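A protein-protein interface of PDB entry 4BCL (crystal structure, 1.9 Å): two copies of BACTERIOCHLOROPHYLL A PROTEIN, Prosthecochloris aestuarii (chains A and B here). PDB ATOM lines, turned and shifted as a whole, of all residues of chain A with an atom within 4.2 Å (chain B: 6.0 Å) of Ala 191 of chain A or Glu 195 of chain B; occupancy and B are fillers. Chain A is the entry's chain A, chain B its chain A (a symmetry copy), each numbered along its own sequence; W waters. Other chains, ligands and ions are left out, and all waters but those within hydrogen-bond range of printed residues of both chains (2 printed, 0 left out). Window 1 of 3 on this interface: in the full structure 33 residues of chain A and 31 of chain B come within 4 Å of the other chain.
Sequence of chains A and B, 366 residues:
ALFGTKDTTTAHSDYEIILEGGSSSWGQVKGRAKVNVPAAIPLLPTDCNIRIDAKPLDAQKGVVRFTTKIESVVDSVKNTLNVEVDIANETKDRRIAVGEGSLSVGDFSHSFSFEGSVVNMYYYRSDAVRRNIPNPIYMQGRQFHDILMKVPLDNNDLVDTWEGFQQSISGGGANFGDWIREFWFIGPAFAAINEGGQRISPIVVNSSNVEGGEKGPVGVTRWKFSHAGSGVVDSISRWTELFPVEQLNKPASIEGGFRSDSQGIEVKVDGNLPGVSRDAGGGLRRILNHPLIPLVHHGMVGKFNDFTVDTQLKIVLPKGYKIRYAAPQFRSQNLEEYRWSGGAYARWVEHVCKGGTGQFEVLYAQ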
ATOM      1  N   PRO A 188      -2.012  10.603  28.133  1.00  0.00           N
ATOM      2  CA  PRO A 188      -2.544  11.738  28.848  1.00  0.00           C
ATOM      3  C   PRO A 188      -1.515  12.230  29.819  1.00  0.00           C
ATOM      4  O   PRO A 188      -1.705  13.260  30.460  1.00  0.00           O
ATOM      5  CB  PRO A 188      -3.772  11.164  29.597  1.00  0.00           C
ATOM      6  CG  PRO A 188      -3.599   9.697  29.551  1.00  0.00           C
ATOM      7  CD  PRO A 188      -2.790   9.381  28.327  1.00  0.00           C
ATOM      8  N   ALA A 189      -0.375  11.555  29.910  1.00  0.00           N
ATOM      9  CA  ALA A 189       0.606  12.116  30.866  1.00  0.00           C
ATOM     10  C   ALA A 189       1.093  13.522  30.462  1.00  0.00           C
ATOM     11  O   ALA A 189       1.313  14.443  31.248  1.00  0.00           O
ATOM     12  CB  ALA A 189       1.764  11.168  30.933  1.00  0.00           C
ATOM     13  N   PHE A 190       1.117  13.785  29.191  1.00  0.00           N
ATOM     14  CA  PHE A 190       1.609  15.090  28.833  1.00  0.00           C
ATOM     15  C   PHE A 190       0.856  16.254  29.367  1.00  0.00           C
ATOM     16  O   PHE A 190       1.313  17.353  29.757  1.00  0.00           O
ATOM     17  CB  PHE A 190       1.628  15.134  27.284  1.00  0.00           C
ATOM     18  CG  PHE A 190       2.413  16.353  26.724  1.00  0.00           C
ATOM     19  CD1 PHE A 190       3.794  16.313  26.494  1.00  0.00           C
ATOM     20  CD2 PHE A 190       1.753  17.553  26.444  1.00  0.00           C
ATOM     21  CE1 PHE A 190       4.425  17.444  25.973  1.00  0.00           C
ATOM     22  CE2 PHE A 190       2.363  18.729  25.996  1.00  0.00           C
ATOM     23  CZ  PHE A 190       3.731  18.640  25.736  1.00  0.00           C
ATOM     24  N   ALA A 191      -0.413  16.049  29.159  1.00  0.00           N
ATOM     25  CA  ALA A 191      -1.273  17.130  29.511  1.00  0.00           C
ATOM     26  C   ALA A 191      -1.279  17.329  31.023  1.00  0.00           C
ATOM     27  O   ALA A 191      -1.501  18.364  31.511  1.00  0.00           O
ATOM     28  CB  ALA A 191      -2.692  16.768  29.033  1.00  0.00           C
ATOM     29  N   ALA A 192      -0.964  16.337  31.794  1.00  0.00           N
ATOM     30  CA  ALA A 192      -0.979  16.541  33.211  1.00  0.00           C
ATOM     31  C   ALA A 192       0.094  17.421  33.755  1.00  0.00           C
ATOM     32  O   ALA A 192       0.037  17.910  34.917  1.00  0.00           O
ATOM     33  CB  ALA A 192      -0.789  15.170  33.849  1.00  0.00           C
ATOM     34  N   ILE A 193       1.145  17.570  32.956  1.00  0.00           N
ATOM     35  CA  ILE A 193       2.303  18.378  33.486  1.00  0.00           C
ATOM     36  C   ILE A 193       1.829  19.784  33.787  1.00  0.00           C
ATOM     37  O   ILE A 193       2.057  20.327  34.881  1.00  0.00           O
ATOM     38  CB  ILE A 193       3.374  18.486  32.355  1.00  0.00           C
ATOM     39  CG1 ILE A 193       3.979  17.111  32.149  1.00  0.00           C
ATOM     40  CG2 ILE A 193       4.448  19.438  32.837  1.00  0.00           C
ATOM     41  CD1 ILE A 193       4.704  16.950  30.806  1.00  0.00           C
ATOM     42  N   ASN A 194       1.257  20.317  32.731  1.00  0.00           N
ATOM     43  CA  ASN A 194       0.798  21.682  32.949  1.00  0.00           C
ATOM     44  C   ASN A 194      -0.290  21.800  34.052  1.00  0.00           C
ATOM     45  O   ASN A 194      -0.325  22.761  34.818  1.00  0.00           O
ATOM     46  CB  ASN A 194       0.203  22.224  31.633  1.00  0.00           C
ATOM     47  CG  ASN A 194       0.061  23.759  31.717  1.00  0.00           C
ATOM     48  OD1 ASN A 194       1.109  24.450  31.750  1.00  0.00           O
ATOM     49  ND2 ASN A 194      -1.163  24.252  31.841  1.00  0.00           N
ATOM     50  N   GLU A 195      -1.133  20.778  34.175  1.00  0.00           N
ATOM     51  CA  GLU A 195      -2.292  20.836  35.113  1.00  0.00           C
ATOM     52  C   GLU A 195      -1.740  20.958  36.486  1.00  0.00           C
ATOM     53  O   GLU A 195      -2.365  21.578  37.331  1.00  0.00           O
ATOM     54  CB  GLU A 195      -2.946  19.452  35.201  1.00  0.00           C
ATOM     55  CG  GLU A 195      -4.100  19.159  34.305  1.00  0.00           C
ATOM     56  CD  GLU A 195      -5.245  20.043  34.616  1.00  0.00           C
ATOM     57  OE1 GLU A 195      -6.062  19.746  35.657  1.00  0.00           O
ATOM     58  OE2 GLU A 195      -5.392  20.947  33.872  1.00  0.00           O
ATOM     59  N   ALA B 191      -6.414  26.534  24.257  1.00  0.00           N
ATOM     60  CA  ALA B 191      -6.230  25.771  25.448  1.00  0.00           C
ATOM     61  C   ALA B 191      -6.458  24.290  25.167  1.00  0.00           C
ATOM     62  O   ALA B 191      -5.946  23.453  25.796  1.00  0.00           O
ATOM     63  CB  ALA B 191      -7.261  26.266  26.480  1.00  0.00           C
ATOM     64  N   ALA B 192      -7.193  23.943  24.157  1.00  0.00           N
ATOM     65  CA  ALA B 192      -7.401  22.548  23.911  1.00  0.00           C
ATOM     66  C   ALA B 192      -6.214  21.787  23.425  1.00  0.00           C
ATOM     67  O   ALA B 192      -6.173  20.526  23.438  1.00  0.00           O
ATOM     68  CB  ALA B 192      -8.461  22.452  22.820  1.00  0.00           C
ATOM     69  N   ILE B 193      -5.254  22.539  22.897  1.00  0.00           N
ATOM     70  CA  ILE B 193      -4.066  21.822  22.307  1.00  0.00           C
ATOM     71  C   ILE B 193      -3.387  21.012  23.393  1.00  0.00           C
ATOM     72  O   ILE B 193      -3.112  19.811  23.231  1.00  0.00           O
ATOM     73  CB  ILE B 193      -3.041  22.898  21.828  1.00  0.00           C
ATOM     74  CG1 ILE B 193      -3.639  23.616  20.633  1.00  0.00           C
ATOM     75  CG2 ILE B 193      -1.786  22.170  21.398  1.00  0.00           C
ATOM     76  CD1 ILE B 193      -2.977  24.967  20.329  1.00  0.00           C
ATOM     77  N   ASN B 194      -3.083  21.774  24.419  1.00  0.00           N
ATOM     78  CA  ASN B 194      -2.407  21.058  25.491  1.00  0.00           C
ATOM     79  C   ASN B 194      -3.266  19.925  26.118  1.00  0.00           C
ATOM     80  O   ASN B 194      -2.762  18.867  26.487  1.00  0.00           O
ATOM     81  CB  ASN B 194      -2.047  22.058  26.609  1.00  0.00           C
ATOM     82  CG  ASN B 194      -1.013  21.425  27.564  1.00  0.00           C
ATOM     83  OD1 ASN B 194       0.144  21.207  27.126  1.00  0.00           O
ATOM     84  ND2 ASN B 194      -1.435  21.064  28.768  1.00  0.00           N
ATOM     85  N   GLU B 195      -4.580  20.128  26.168  1.00  0.00           N
ATOM     86  CA  GLU B 195      -5.488  19.167  26.860  1.00  0.00           C
ATOM     87  C   GLU B 195      -5.394  17.875  26.137  1.00  0.00           C
ATOM     88  O   GLU B 195      -5.529  16.831  26.753  1.00  0.00           O
ATOM     89  CB  GLU B 195      -6.945  19.542  26.568  1.00  0.00           C
ATOM     90  CG  GLU B 195      -7.658  20.417  27.541  1.00  0.00           C
ATOM     91  CD  GLU B 195      -7.787  19.747  28.854  1.00  0.00           C
ATOM     92  OE1 GLU B 195      -8.772  18.836  29.051  1.00  0.00           O
ATOM     93  OE2 GLU B 195      -7.022  20.109  29.676  1.00  0.00           O
ATOM     94  N   GLY B 196      -5.146  17.962  24.852  1.00  0.00           N
ATOM     95  CA  GLY B 196      -4.998  16.784  23.997  1.00  0.00           C
ATOM     96  C   GLY B 196      -3.585  16.175  24.029  1.00  0.00           C
ATOM     97  O   GLY B 196      -3.295  15.209  23.372  1.00  0.00           O
ATOM     98  N   GLY B 197      -2.644  16.793  24.757  1.00  0.00           N
ATOM     99  CA  GLY B 197      -1.232  16.303  24.768  1.00  0.00           C
ATOM    100  C   GLY B 197      -0.716  16.553  23.348  1.00  0.00           C
ATOM    101  O   GLY B 197       0.131  15.849  22.851  1.00  0.00           O
ATOM    102  N   GLN B 198      -1.136  17.670  22.758  1.00  0.00           N
ATOM    103  CA  GLN B 198      -0.715  17.954  21.423  1.00  0.00           C
ATOM    104  C   GLN B 198       0.241  19.119  21.437  1.00  0.00           C
ATOM    105  O   GLN B 198       0.279  19.891  22.390  1.00  0.00           O
ATOM    106  CB  GLN B 198      -1.980  18.361  20.609  1.00  0.00           C
ATOM    107  CG  GLN B 198      -1.748  18.522  19.081  1.00  0.00           C
ATOM    108  CD  GLN B 198      -3.027  18.536  18.256  1.00  0.00           C
ATOM    109  OE1 GLN B 198      -3.064  18.405  17.013  1.00  0.00           O
ATOM    110  NE2 GLN B 198      -4.138  18.738  18.919  1.00  0.00           N
ATOM    111  N   SER B 230       1.427  13.069  22.034  1.00  0.00           N
ATOM    112  CA  SER B 230       1.924  12.046  22.945  1.00  0.00           C
ATOM    113  C   SER B 230       1.164  10.740  22.794  1.00  0.00           C
ATOM    114  O   SER B 230       1.389   9.763  23.464  1.00  0.00           O
ATOM    115  CB  SER B 230       1.860  12.449  24.382  1.00  0.00           C
ATOM    116  OG  SER B 230       0.511  12.765  24.600  1.00  0.00           O
ATOM    117  N   VAL B 232      -2.481  10.763  22.152  1.00  0.00           N
ATOM    118  CA  VAL B 232      -3.931  10.848  22.209  1.00  0.00           C
ATOM    119  C   VAL B 232      -4.390  11.429  20.911  1.00  0.00           C
ATOM    120  O   VAL B 232      -5.533  11.245  20.479  1.00  0.00           O
ATOM    121  CB  VAL B 232      -4.352  11.771  23.385  1.00  0.00           C
ATOM    122  CG1 VAL B 232      -5.804  12.224  23.375  1.00  0.00           C
ATOM    123  CG2 VAL B 232      -3.968  11.236  24.774  1.00  0.00           C
ATOM    124  N   VAL B 296     -11.802  13.852  24.490  1.00  0.00           N
ATOM    125  CA  VAL B 296     -11.070  14.768  25.349  1.00  0.00           C
ATOM    126  C   VAL B 296     -11.492  16.188  25.064  1.00  0.00           C
ATOM    127  O   VAL B 296     -11.585  16.978  25.971  1.00  0.00           O
ATOM    128  CB  VAL B 296      -9.561  14.596  25.086  1.00  0.00           C
ATOM    129  CG1 VAL B 296      -8.854  15.698  25.918  1.00  0.00           C
ATOM    130  CG2 VAL B 296      -9.142  13.163  25.568  1.00  0.00           C
ATOM    131  N   HIS B 297     -11.734  16.557  23.803  1.00  0.00           N
ATOM    132  CA  HIS B 297     -12.042  17.945  23.615  1.00  0.00           C
ATOM    133  C   HIS B 297     -13.509  18.220  24.015  1.00  0.00           C
ATOM    134  O   HIS B 297     -13.858  19.223  24.588  1.00  0.00           O
ATOM    135  CB  HIS B 297     -11.981  18.103  22.084  1.00  0.00           C
ATOM    136  CG  HIS B 297     -10.554  18.389  21.665  1.00  0.00           C
ATOM    137  ND1 HIS B 297     -10.301  18.933  20.448  1.00  0.00           N
ATOM    138  CD2 HIS B 297      -9.320  18.253  22.359  1.00  0.00           C
ATOM    139  CE1 HIS B 297      -8.969  19.010  20.309  1.00  0.00           C
ATOM    140  NE2 HIS B 297      -8.346  18.675  21.423  1.00  0.00           N
ATOM    141  N   GLY B 299     -14.850  16.729  26.262  1.00  0.00           N
ATOM    142  CA  GLY B 299     -14.751  16.705  27.731  1.00  0.00           C
ATOM    143  C   GLY B 299     -14.647  18.122  28.308  1.00  0.00           C
ATOM    144  O   GLY B 299     -15.017  18.382  29.480  1.00  0.00           O
ATOM    145  N   MET B 300     -14.152  19.089  27.507  1.00  0.00           N
ATOM    146  CA  MET B 300     -14.026  20.456  27.999  1.00  0.00           C
ATOM    147  C   MET B 300     -15.344  21.157  28.092  1.00  0.00           C
ATOM    148  O   MET B 300     -15.387  22.183  28.671  1.00  0.00           O
ATOM    149  CB  MET B 300     -13.078  21.258  27.051  1.00  0.00           C
ATOM    150  CG  MET B 300     -11.702  20.498  27.081  1.00  0.00           C
ATOM    151  SD  MET B 300     -10.443  21.345  26.006  1.00  0.00           S
ATOM    152  CE  MET B 300     -10.088  22.819  26.924  1.00  0.00           C
HETATM  153  O   HOH W   1       1.300  19.954  29.733  1.00  0.00           O
HETATM  154  O   HOH W   2      -7.447  21.489  32.060  1.00  0.00           O
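Ala 191 of chain A touches just these residues of chain B: Asn 194 (3.3 Å) and Glu 195 (3.6 Å).
Printed residues of chain B within 4 Å of Asn 194 of chain A: Asn 194 (3.5 Å).
Printed residues of chain A within 4 Å of Gly 197 of chain B: Phe 190.
Of the printed residues of chain A, Ser 230 of chain B touches Phe 190 (3.8 Å).
Of the printed residues of chain A, Val 232 of chain B touches Pro 188.
The nearest residue of chain B that does not touch Ala 191 of chain A is Gly 197 of chain B (4.3 Å).
Of the 8 printed residues of chain A, 4 touch a printed residue of chain B.
Of the 14 printed residues of chain B, 5 touch a printed residue of chain A.
Among the printed residues, no Asp or Glu carboxylate lies within 4 Å of a Lys or Arg side-chain nitrogen of the other chain.
Ala 191 of chain A touches Asn 194 of chain B, but with the chains exchanged Asn 194 of chain A does not touch Ala 191 of chain B (7.7 Å).
Ala 191 of chain A touches Glu 195 of chain B, but with the chains exchanged Glu 195 of chain A does not touch Ala 191 of chain B (8.5 Å).
Asn 194 of chain B touches its own counterpart, Asn 194 of chain A.
Of the 7 pairs that touch across the chains among the printed residues, 1 has its exchanged pair printed and touching as well.
Water W1 lies within hydrogen-bond range of the backbone carbonyl oxygen of Phe 190 of chain A (2.6 Å), the backbone NH of Asn 194 of chain A (3.0 Å) and the side-chain amide nitrogen of Asn 194 of chain B (3.1 Å).
Water W2 bridges the side-chain carboxylate of Glu 195 of chain B and the side-chain carboxylate of Glu 195 of chain A.
O of Gly 197 of chain B sits at hydrogen-bond distance from N of Ser 230 of chain B, 3.2 Å away.
Among the printed residues, merely in contact across the chains: Ala 191 of chain A with Asn 194 of chain B, Asn 194 of chain A with Asn 194 of chain B, Phe 190 of chain A with Asn 194 of chain B, Ala 191 of chain A with Glu 195 of chain B, Phe 190 of chain A with Gly 197 of chain B, Phe 190 of chain A with Ser 230 of chain B and Pro 188 of chain A with Val 232 of chain B.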
